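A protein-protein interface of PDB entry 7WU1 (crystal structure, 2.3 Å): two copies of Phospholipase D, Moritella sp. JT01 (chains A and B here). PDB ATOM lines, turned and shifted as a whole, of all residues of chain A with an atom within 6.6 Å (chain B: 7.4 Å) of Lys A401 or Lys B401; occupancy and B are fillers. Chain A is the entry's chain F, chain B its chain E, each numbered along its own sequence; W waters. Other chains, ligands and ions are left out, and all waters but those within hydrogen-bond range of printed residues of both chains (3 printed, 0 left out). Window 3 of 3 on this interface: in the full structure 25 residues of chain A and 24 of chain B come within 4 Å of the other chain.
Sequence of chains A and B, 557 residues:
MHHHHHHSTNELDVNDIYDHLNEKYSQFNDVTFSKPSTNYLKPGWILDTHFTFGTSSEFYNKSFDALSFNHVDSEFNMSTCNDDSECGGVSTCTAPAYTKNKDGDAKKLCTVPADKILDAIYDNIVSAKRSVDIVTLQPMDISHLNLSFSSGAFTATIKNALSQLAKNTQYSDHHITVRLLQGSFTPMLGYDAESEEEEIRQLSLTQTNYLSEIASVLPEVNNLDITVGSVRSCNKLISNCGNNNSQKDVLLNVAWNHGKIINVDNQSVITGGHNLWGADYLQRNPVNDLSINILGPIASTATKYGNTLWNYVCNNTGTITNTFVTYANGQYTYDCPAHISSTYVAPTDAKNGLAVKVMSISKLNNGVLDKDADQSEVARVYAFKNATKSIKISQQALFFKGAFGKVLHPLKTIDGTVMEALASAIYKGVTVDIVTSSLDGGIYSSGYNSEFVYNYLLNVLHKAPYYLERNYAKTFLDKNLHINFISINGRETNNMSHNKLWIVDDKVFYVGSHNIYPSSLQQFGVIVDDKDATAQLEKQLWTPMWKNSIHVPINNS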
ATOM      1  N   ASP A 249       8.783 -17.977   0.492  1.00  0.00           N
ATOM      2  CA  ASP A 249       9.582 -17.365  -0.554  1.00  0.00           C
ATOM      3  C   ASP A 249      10.334 -16.196   0.061  1.00  0.00           C
ATOM      4  O   ASP A 249       9.871 -15.570   1.024  1.00  0.00           O
ATOM      5  CB  ASP A 249       8.710 -16.923  -1.733  1.00  0.00           C
ATOM      6  CG  ASP A 249       9.541 -16.599  -2.979  1.00  0.00           C
ATOM      7  OD1 ASP A 249      10.042 -15.444  -3.066  1.00  0.00           O
ATOM      8  OD2 ASP A 249       9.720 -17.501  -3.856  1.00  0.00           O
ATOM      9  N   LEU A 251      10.750 -13.315  -1.177  1.00  0.00           N
ATOM     10  CA  LEU A 251      10.019 -12.072  -1.378  1.00  0.00           C
ATOM     11  C   LEU A 251       8.838 -11.919  -0.434  1.00  0.00           C
ATOM     12  O   LEU A 251       8.237 -10.839  -0.399  1.00  0.00           O
ATOM     13  CB  LEU A 251       9.539 -11.984  -2.825  1.00  0.00           C
ATOM     14  CG  LEU A 251      10.657 -11.986  -3.870  1.00  0.00           C
ATOM     15  CD1 LEU A 251      10.083 -11.723  -5.290  1.00  0.00           C
ATOM     16  CD2 LEU A 251      11.730 -10.985  -3.536  1.00  0.00           C
ATOM     17  N   PHE A 399      -1.516 -13.494  -9.369  1.00  0.00           N
ATOM     18  CA  PHE A 399      -0.381 -14.277  -8.913  1.00  0.00           C
ATOM     19  C   PHE A 399       0.845 -13.371  -8.877  1.00  0.00           C
ATOM     20  O   PHE A 399       0.853 -12.262  -9.424  1.00  0.00           O
ATOM     21  CB  PHE A 399      -0.131 -15.497  -9.812  1.00  0.00           C
ATOM     22  CG  PHE A 399      -1.285 -16.455  -9.861  1.00  0.00           C
ATOM     23  CD1 PHE A 399      -2.338 -16.239 -10.717  1.00  0.00           C
ATOM     24  CD2 PHE A 399      -1.314 -17.567  -9.037  1.00  0.00           C
ATOM     25  CE1 PHE A 399      -3.399 -17.105 -10.762  1.00  0.00           C
ATOM     26  CE2 PHE A 399      -2.383 -18.457  -9.071  1.00  0.00           C
ATOM     27  CZ  PHE A 399      -3.428 -18.225  -9.931  1.00  0.00           C
ATOM     28  N   PHE A 400       1.899 -13.850  -8.225  1.00  0.00           N
ATOM     29  CA  PHE A 400       3.096 -13.044  -8.052  1.00  0.00           C
ATOM     30  C   PHE A 400       4.321 -13.936  -8.157  1.00  0.00           C
ATOM     31  O   PHE A 400       4.389 -14.999  -7.522  1.00  0.00           O
ATOM     32  CB  PHE A 400       3.052 -12.316  -6.693  1.00  0.00           C
ATOM     33  CG  PHE A 400       4.213 -11.400  -6.455  1.00  0.00           C
ATOM     34  CD1 PHE A 400       4.237 -10.132  -7.006  1.00  0.00           C
ATOM     35  CD2 PHE A 400       5.276 -11.811  -5.675  1.00  0.00           C
ATOM     36  CE1 PHE A 400       5.323  -9.275  -6.789  1.00  0.00           C
ATOM     37  CE2 PHE A 400       6.360 -10.966  -5.449  1.00  0.00           C
ATOM     38  CZ  PHE A 400       6.378  -9.688  -6.016  1.00  0.00           C
ATOM     39  N   LYS A 401       5.299 -13.479  -8.928  1.00  0.00           N
ATOM     40  CA  LYS A 401       6.509 -14.252  -9.177  1.00  0.00           C
ATOM     41  C   LYS A 401       7.447 -14.130  -7.988  1.00  0.00           C
ATOM     42  O   LYS A 401       7.859 -13.016  -7.636  1.00  0.00           O
ATOM     43  CB  LYS A 401       7.176 -13.744 -10.460  1.00  0.00           C
ATOM     44  CG  LYS A 401       8.429 -14.488 -10.880  1.00  0.00           C
ATOM     45  CD  LYS A 401       9.477 -13.565 -11.551  1.00  0.00           C
ATOM     46  CE  LYS A 401       9.912 -12.398 -10.612  1.00  0.00           C
ATOM     47  NZ  LYS A 401      10.898 -12.718  -9.516  1.00  0.00           N
ATOM     48  N   GLY A 402       7.796 -15.271  -7.395  1.00  0.00           N
ATOM     49  CA  GLY A 402       8.715 -15.306  -6.281  1.00  0.00           C
ATOM     50  C   GLY A 402      10.147 -15.065  -6.709  1.00  0.00           C
ATOM     51  O   GLY A 402      10.462 -14.873  -7.885  1.00  0.00           O
ATOM     52  N   ALA A 403      11.046 -15.152  -5.726  1.00  0.00           N
ATOM     53  CA  ALA A 403      12.421 -14.704  -5.925  1.00  0.00           C
ATOM     54  C   ALA A 403      13.134 -15.450  -7.040  1.00  0.00           C
ATOM     55  O   ALA A 403      13.963 -14.864  -7.745  1.00  0.00           O
ATOM     56  CB  ALA A 403      13.202 -14.857  -4.628  1.00  0.00           C
ATOM     57  N   PHE A 404      12.859 -16.740  -7.205  1.00  0.00           N
ATOM     58  CA  PHE A 404      13.555 -17.568  -8.189  1.00  0.00           C
ATOM     59  C   PHE A 404      12.582 -18.139  -9.211  1.00  0.00           C
ATOM     60  O   PHE A 404      12.810 -19.194  -9.791  1.00  0.00           O
ATOM     61  CB  PHE A 404      14.349 -18.669  -7.480  1.00  0.00           C
ATOM     62  CG  PHE A 404      15.259 -18.139  -6.405  1.00  0.00           C
ATOM     63  CD1 PHE A 404      16.221 -17.202  -6.704  1.00  0.00           C
ATOM     64  CD2 PHE A 404      15.107 -18.521  -5.103  1.00  0.00           C
ATOM     65  CE1 PHE A 404      17.033 -16.666  -5.735  1.00  0.00           C
ATOM     66  CE2 PHE A 404      15.934 -17.987  -4.107  1.00  0.00           C
ATOM     67  CZ  PHE A 404      16.904 -17.061  -4.436  1.00  0.00           C
ATOM     68  N   GLY A 405      11.499 -17.433  -9.452  1.00  0.00           N
ATOM     69  CA  GLY A 405      10.571 -17.800 -10.495  1.00  0.00           C
ATOM     70  C   GLY A 405       9.362 -18.587 -10.040  1.00  0.00           C
ATOM     71  O   GLY A 405       8.434 -18.781 -10.834  1.00  0.00           O
ATOM     72  N   LYS A 406       9.337 -19.047  -8.796  1.00  0.00           N
ATOM     73  CA  LYS A 406       8.186 -19.796  -8.324  1.00  0.00           C
ATOM     74  C   LYS A 406       6.944 -18.914  -8.357  1.00  0.00           C
ATOM     75  O   LYS A 406       6.976 -17.766  -7.906  1.00  0.00           O
ATOM     76  CB  LYS A 406       8.427 -20.294  -6.906  1.00  0.00           C
ATOM     77  CG  LYS A 406       7.278 -21.097  -6.351  1.00  0.00           C
ATOM     78  CD  LYS A 406       7.118 -22.407  -7.121  1.00  0.00           C
ATOM     79  CE  LYS A 406       5.937 -23.236  -6.597  1.00  0.00           C
ATOM     80  NZ  LYS A 406       4.612 -22.607  -6.954  1.00  0.00           N
ATOM     81  N   VAL A 407       5.845 -19.460  -8.870  1.00  0.00           N
ATOM     82  CA  VAL A 407       4.565 -18.761  -8.816  1.00  0.00           C
ATOM     83  C   VAL A 407       4.020 -18.827  -7.397  1.00  0.00           C
ATOM     84  O   VAL A 407       3.832 -19.919  -6.844  1.00  0.00           O
ATOM     85  CB  VAL A 407       3.562 -19.366  -9.801  1.00  0.00           C
ATOM     86  CG1 VAL A 407       2.316 -18.488  -9.881  1.00  0.00           C
ATOM     87  CG2 VAL A 407       4.174 -19.501 -11.144  1.00  0.00           C
ATOM     88  N   LEU A 408       3.750 -17.657  -6.816  1.00  0.00           N
ATOM     89  CA  LEU A 408       3.101 -17.551  -5.513  1.00  0.00           C
ATOM     90  C   LEU A 408       1.620 -17.233  -5.706  1.00  0.00           C
ATOM     91  O   LEU A 408       1.271 -16.308  -6.452  1.00  0.00           O
ATOM     92  CB  LEU A 408       3.771 -16.468  -4.672  1.00  0.00           C
ATOM     93  CG  LEU A 408       5.288 -16.619  -4.571  1.00  0.00           C
ATOM     94  CD1 LEU A 408       5.856 -15.499  -3.707  1.00  0.00           C
ATOM     95  CD2 LEU A 408       5.647 -18.012  -4.030  1.00  0.00           C
ATOM     96  N   GLY A 447       1.632  -9.918 -14.804  1.00  0.00           N
ATOM     97  CA  GLY A 447       2.581 -10.948 -14.440  1.00  0.00           C
ATOM     98  C   GLY A 447       2.382 -12.297 -15.103  1.00  0.00           C
ATOM     99  O   GLY A 447       3.346 -13.009 -15.396  1.00  0.00           O
ATOM    100  N   TYR A 448       1.128 -12.666 -15.319  1.00  0.00           N
ATOM    101  CA  TYR A 448       0.755 -13.947 -15.895  1.00  0.00           C
ATOM    102  C   TYR A 448      -0.389 -13.730 -16.867  1.00  0.00           C
ATOM    103  O   TYR A 448      -1.226 -12.840 -16.691  1.00  0.00           O
ATOM    104  CB  TYR A 448       0.372 -14.946 -14.789  1.00  0.00           C
ATOM    105  CG  TYR A 448       1.524 -15.200 -13.839  1.00  0.00           C
ATOM    106  CD1 TYR A 448       2.420 -16.225 -14.075  1.00  0.00           C
ATOM    107  CD2 TYR A 448       1.749 -14.378 -12.736  1.00  0.00           C
ATOM    108  CE1 TYR A 448       3.510 -16.438 -13.232  1.00  0.00           C
ATOM    109  CE2 TYR A 448       2.840 -14.583 -11.895  1.00  0.00           C
ATOM    110  CZ  TYR A 448       3.709 -15.620 -12.150  1.00  0.00           C
ATOM    111  OH  TYR A 448       4.776 -15.866 -11.319  1.00  0.00           O
ATOM    112  N   ASP B 249      21.155  -5.692  -4.984  1.00  0.00           N
ATOM    113  CA  ASP B 249      19.804  -6.243  -4.989  1.00  0.00           C
ATOM    114  C   ASP B 249      19.818  -7.577  -4.266  1.00  0.00           C
ATOM    115  O   ASP B 249      20.801  -8.318  -4.344  1.00  0.00           O
ATOM    116  CB  ASP B 249      19.275  -6.415  -6.421  1.00  0.00           C
ATOM    117  CG  ASP B 249      17.774  -6.585  -6.466  1.00  0.00           C
ATOM    118  OD1 ASP B 249      17.050  -5.556  -6.468  1.00  0.00           O
ATOM    119  OD2 ASP B 249      17.328  -7.748  -6.478  1.00  0.00           O
ATOM    120  N   LEU B 251      18.337 -10.224  -4.995  1.00  0.00           N
ATOM    121  CA  LEU B 251      18.402 -11.325  -5.935  1.00  0.00           C
ATOM    122  C   LEU B 251      19.783 -11.525  -6.533  1.00  0.00           C
ATOM    123  O   LEU B 251      20.036 -12.593  -7.105  1.00  0.00           O
ATOM    124  CB  LEU B 251      17.373 -11.108  -7.048  1.00  0.00           C
ATOM    125  CG  LEU B 251      15.929 -11.147  -6.553  1.00  0.00           C
ATOM    126  CD1 LEU B 251      14.942 -11.071  -7.709  1.00  0.00           C
ATOM    127  CD2 LEU B 251      15.635 -12.399  -5.704  1.00  0.00           C
ATOM    128  N   PHE B 399      17.590  -7.696 -19.454  1.00  0.00           N
ATOM    129  CA  PHE B 399      17.428  -7.055 -18.157  1.00  0.00           C
ATOM    130  C   PHE B 399      16.729  -8.042 -17.246  1.00  0.00           C
ATOM    131  O   PHE B 399      16.090  -8.988 -17.714  1.00  0.00           O
ATOM    132  CB  PHE B 399      16.613  -5.746 -18.283  1.00  0.00           C
ATOM    133  CG  PHE B 399      17.288  -4.689 -19.139  1.00  0.00           C
ATOM    134  CD1 PHE B 399      17.076  -4.646 -20.508  1.00  0.00           C
ATOM    135  CD2 PHE B 399      18.157  -3.761 -18.568  1.00  0.00           C
ATOM    136  CE1 PHE B 399      17.680  -3.705 -21.284  1.00  0.00           C
ATOM    137  CE2 PHE B 399      18.782  -2.803 -19.353  1.00  0.00           C
ATOM    138  CZ  PHE B 399      18.541  -2.783 -20.725  1.00  0.00           C
ATOM    139  N   PHE B 400      16.841  -7.810 -15.939  1.00  0.00           N
ATOM    140  CA  PHE B 400      16.288  -8.722 -14.939  1.00  0.00           C
ATOM    141  C   PHE B 400      15.628  -7.930 -13.820  1.00  0.00           C
ATOM    142  O   PHE B 400      16.214  -6.957 -13.329  1.00  0.00           O
ATOM    143  CB  PHE B 400      17.381  -9.630 -14.371  1.00  0.00           C
ATOM    144  CG  PHE B 400      16.874 -10.693 -13.448  1.00  0.00           C
ATOM    145  CD1 PHE B 400      16.355 -11.882 -13.944  1.00  0.00           C
ATOM    146  CD2 PHE B 400      16.949 -10.531 -12.062  1.00  0.00           C
ATOM    147  CE1 PHE B 400      15.909 -12.887 -13.065  1.00  0.00           C
ATOM    148  CE2 PHE B 400      16.504 -11.539 -11.197  1.00  0.00           C
ATOM    149  CZ  PHE B 400      15.974 -12.703 -11.702  1.00  0.00           C
ATOM    150  N   LYS B 401      14.425  -8.356 -13.418  1.00  0.00           N
ATOM    151  CA  LYS B 401      13.661  -7.655 -12.390  1.00  0.00           C
ATOM    152  C   LYS B 401      14.191  -8.010 -11.004  1.00  0.00           C
ATOM    153  O   LYS B 401      14.203  -9.182 -10.606  1.00  0.00           O
ATOM    154  CB  LYS B 401      12.174  -7.991 -12.482  1.00  0.00           C
ATOM    155  CG  LYS B 401      11.307  -7.239 -11.486  1.00  0.00           C
ATOM    156  CD  LYS B 401       9.796  -7.295 -11.821  1.00  0.00           C
ATOM    157  CE  LYS B 401       9.158  -8.592 -11.302  1.00  0.00           C
ATOM    158  NZ  LYS B 401       7.644  -8.519 -11.296  1.00  0.00           N
ATOM    159  N   GLY B 402      14.622  -6.995 -10.264  1.00  0.00           N
ATOM    160  CA  GLY B 402      15.067  -7.162  -8.905  1.00  0.00           C
ATOM    161  C   GLY B 402      13.930  -7.432  -7.948  1.00  0.00           C
ATOM    162  O   GLY B 402      12.753  -7.481  -8.308  1.00  0.00           O
ATOM    163  N   ALA B 403      14.313  -7.587  -6.680  1.00  0.00           N
ATOM    164  CA  ALA B 403      13.406  -8.137  -5.683  1.00  0.00           C
ATOM    165  C   ALA B 403      12.152  -7.292  -5.497  1.00  0.00           C
ATOM    166  O   ALA B 403      11.069  -7.822  -5.215  1.00  0.00           O
ATOM    167  CB  ALA B 403      14.154  -8.272  -4.368  1.00  0.00           C
ATOM    168  N   PHE B 404      12.272  -5.990  -5.608  1.00  0.00           N
ATOM    169  CA  PHE B 404      11.156  -5.083  -5.402  1.00  0.00           C
ATOM    170  C   PHE B 404      10.875  -4.244  -6.641  1.00  0.00           C
ATOM    171  O   PHE B 404      10.349  -3.129  -6.571  1.00  0.00           O
ATOM    172  CB  PHE B 404      11.463  -4.241  -4.183  1.00  0.00           C
ATOM    173  CG  PHE B 404      11.861  -5.075  -3.004  1.00  0.00           C
ATOM    174  CD1 PHE B 404      11.001  -6.054  -2.522  1.00  0.00           C
ATOM    175  CD2 PHE B 404      13.104  -4.928  -2.408  1.00  0.00           C
ATOM    176  CE1 PHE B 404      11.352  -6.846  -1.467  1.00  0.00           C
ATOM    177  CE2 PHE B 404      13.477  -5.734  -1.339  1.00  0.00           C
ATOM    178  CZ  PHE B 404      12.595  -6.685  -0.864  1.00  0.00           C
ATOM    179  N   GLY B 405      11.192  -4.795  -7.797  1.00  0.00           N
ATOM    180  CA  GLY B 405      10.815  -4.202  -9.054  1.00  0.00           C
ATOM    181  C   GLY B 405      11.878  -3.376  -9.729  1.00  0.00           C
ATOM    182  O   GLY B 405      11.665  -2.958 -10.880  1.00  0.00           O
ATOM    183  N   LYS B 406      12.989  -3.107  -9.045  1.00  0.00           N
ATOM    184  CA  LYS B 406      14.092  -2.392  -9.664  1.00  0.00           C
ATOM    185  C   LYS B 406      14.614  -3.149 -10.874  1.00  0.00           C
ATOM    186  O   LYS B 406      14.824  -4.355 -10.821  1.00  0.00           O
ATOM    187  CB  LYS B 406      15.219  -2.193  -8.665  1.00  0.00           C
ATOM    188  CG  LYS B 406      16.388  -1.413  -9.235  1.00  0.00           C
ATOM    189  CD  LYS B 406      15.964   0.033  -9.561  1.00  0.00           C
ATOM    190  CE  LYS B 406      17.118   0.842 -10.137  1.00  0.00           C
ATOM    191  NZ  LYS B 406      17.339   0.563 -11.576  1.00  0.00           N
ATOM    192  N   VAL B 407      14.811  -2.441 -11.970  1.00  0.00           N
ATOM    193  CA  VAL B 407      15.405  -3.042 -13.161  1.00  0.00           C
ATOM    194  C   VAL B 407      16.904  -3.197 -12.950  1.00  0.00           C
ATOM    195  O   VAL B 407      17.600  -2.230 -12.616  1.00  0.00           O
ATOM    196  CB  VAL B 407      15.133  -2.199 -14.421  1.00  0.00           C
ATOM    197  CG1 VAL B 407      15.726  -2.928 -15.650  1.00  0.00           C
ATOM    198  CG2 VAL B 407      13.676  -1.917 -14.601  1.00  0.00           C
ATOM    199  N   LEU B 408      17.404  -4.409 -13.139  1.00  0.00           N
ATOM    200  CA  LEU B 408      18.822  -4.693 -13.082  1.00  0.00           C
ATOM    201  C   LEU B 408      19.348  -4.855 -14.498  1.00  0.00           C
ATOM    202  O   LEU B 408      18.751  -5.581 -15.297  1.00  0.00           O
ATOM    203  CB  LEU B 408      19.053  -5.960 -12.274  1.00  0.00           C
ATOM    204  CG  LEU B 408      18.437  -5.969 -10.879  1.00  0.00           C
ATOM    205  CD1 LEU B 408      18.798  -7.288 -10.163  1.00  0.00           C
ATOM    206  CD2 LEU B 408      18.893  -4.775 -10.060  1.00  0.00           C
ATOM    207  N   GLY B 447      10.914 -10.574 -20.030  1.00  0.00           N
ATOM    208  CA  GLY B 447      10.804  -9.715 -18.862  1.00  0.00           C
ATOM    209  C   GLY B 447      10.511  -8.241 -19.130  1.00  0.00           C
ATOM    210  O   GLY B 447       9.888  -7.561 -18.308  1.00  0.00           O
ATOM    211  N   TYR B 448      10.968  -7.727 -20.275  1.00  0.00           N
ATOM    212  CA  TYR B 448      10.799  -6.330 -20.657  1.00  0.00           C
ATOM    213  C   TYR B 448      10.539  -6.269 -22.150  1.00  0.00           C
ATOM    214  O   TYR B 448      11.038  -7.105 -22.916  1.00  0.00           O
ATOM    215  CB  TYR B 448      12.031  -5.508 -20.276  1.00  0.00           C
ATOM    216  CG  TYR B 448      12.280  -5.521 -18.782  1.00  0.00           C
ATOM    217  CD1 TYR B 448      11.747  -4.530 -17.969  1.00  0.00           C
ATOM    218  CD2 TYR B 448      13.023  -6.517 -18.187  1.00  0.00           C
ATOM    219  CE1 TYR B 448      11.932  -4.540 -16.611  1.00  0.00           C
ATOM    220  CE2 TYR B 448      13.231  -6.520 -16.812  1.00  0.00           C
ATOM    221  CZ  TYR B 448      12.683  -5.531 -16.027  1.00  0.00           C
ATOM    222  OH  TYR B 448      12.892  -5.512 -14.671  1.00  0.00           O
ATOM    223  N   TYR B 517      21.513 -10.651 -19.356  1.00  0.00           N
ATOM    224  CA  TYR B 517      20.887 -10.120 -18.152  1.00  0.00           C
ATOM    225  C   TYR B 517      21.719 -10.558 -16.941  1.00  0.00           C
ATOM    226  O   TYR B 517      22.412 -11.590 -16.977  1.00  0.00           O
ATOM    227  CB  TYR B 517      19.415 -10.554 -18.025  1.00  0.00           C
ATOM    228  CG  TYR B 517      19.128 -11.990 -17.635  1.00  0.00           C
ATOM    229  CD1 TYR B 517      19.305 -12.428 -16.313  1.00  0.00           C
ATOM    230  CD2 TYR B 517      18.657 -12.898 -18.556  1.00  0.00           C
ATOM    231  CE1 TYR B 517      19.034 -13.727 -15.954  1.00  0.00           C
ATOM    232  CE2 TYR B 517      18.398 -14.195 -18.203  1.00  0.00           C
ATOM    233  CZ  TYR B 517      18.567 -14.611 -16.910  1.00  0.00           C
ATOM    234  OH  TYR B 517      18.296 -15.906 -16.541  1.00  0.00           O
ATOM    235  N   PRO B 518      21.682  -9.781 -15.859  1.00  0.00           N
ATOM    236  CA  PRO B 518      22.646  -9.982 -14.781  1.00  0.00           C
ATOM    237  C   PRO B 518      22.226 -11.038 -13.770  1.00  0.00           C
ATOM    238  O   PRO B 518      21.040 -11.209 -13.464  1.00  0.00           O
ATOM    239  CB  PRO B 518      22.704  -8.593 -14.126  1.00  0.00           C
ATOM    240  CG  PRO B 518      21.356  -8.029 -14.350  1.00  0.00           C
ATOM    241  CD  PRO B 518      20.980  -8.490 -15.721  1.00  0.00           C
HETATM  242  O   HOH W   1      12.827 -11.490 -11.496  1.00  0.00           O
HETATM  243  O   HOH W   2      11.474  -9.707  -9.300  1.00  0.00           O
HETATM  244  O   HOH W   3       8.121 -10.580  -8.700  1.00  0.00           O
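Of the printed residues of chain B, Leu A251 touches Ala B403.
Printed residues of chain B within 4 Å of Lys A401: Lys B401.
No residue of chain B comes within 4 Å of Gly A402.
Of chain A, only Lys A401 comes within 4 Å of Lys B401.
Of the printed residues of chain A, Ala B403 touches Leu A251 (3.6 Å).
The nearest residue of chain B that does not touch Lys A401 is Leu B251 (4.7 Å).
The nearest residue of chain A that does not touch Lys B401 is Phe A400 (5.1 Å).
Among the printed residues, pairs that only touch across the chains: Ala A403 with Leu B251 (3.6 Å), Leu A251 with Ala B403 (3.6 Å) and Lys A401 with Lys B401 (3.9 Å).
Water W3 bridges O of Lys A401 (2.7 Å) and NZ of Lys B401 (3.3 Å).
Water W2 lies within hydrogen-bond range of the backbone carbonyl oxygen (O) of Gly B402 (2.8 Å), the backbone carbonyl oxygen (O) of Lys B401 (3.1 Å) and the side-chain amino group (NZ) of Lys A401 (3.1 Å).
Water W1 lies within hydrogen-bond range of the backbone carbonyl oxygen (O) of Lys B401 and the side-chain amino group (NZ) of Lys A401.
Of the 14 printed residues of chain A, 3 touch a printed residue of chain B.
Printed residues of chain A that touch a printed residue of chain B: Leu A251, Lys A401 and Ala A403.
Of the 16 printed residues of chain B, 3 touch a printed residue of chain A.
Hydrophobic or aromatic side chains of chain B within 4 Å of the printed part of chain A: Leu B251 and Ala B403.
Among the printed residues, no Asp or Glu carboxylate lies within 4 Å of a Lys or Arg side-chain nitrogen of the other chain.
Leu A251 touches Ala B403, and with the chains exchanged Ala A403 touches Leu B251.
Lys B401 touches its own counterpart, Lys A401.
The backbone NH of Lys B401 lies close to the side-chain hydroxyl of Tyr B448, at 3.5 Å.
The backbone NH (N) of Ala B403 sits at hydrogen-bond distance from the side-chain carboxylate (OD2) of Asp B249 (3.0 Å).
The backbone NH (N) of Lys A401 sits close to the side-chain hydroxyl (OH) of Tyr A448 (3.4 Å).
The side-chain carboxylate (OD2) of Asp B249 lies within hydrogen-bond range of the backbone NH (N) of Leu B251 (3.1 Å).
OD1 of Asp A249 lies within hydrogen-bond range of N of Ala A403, at 2.9 Å.
The side-chain carboxylate of Asp A249 is in hydrogen-bond range of the backbone NH of Leu A251.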
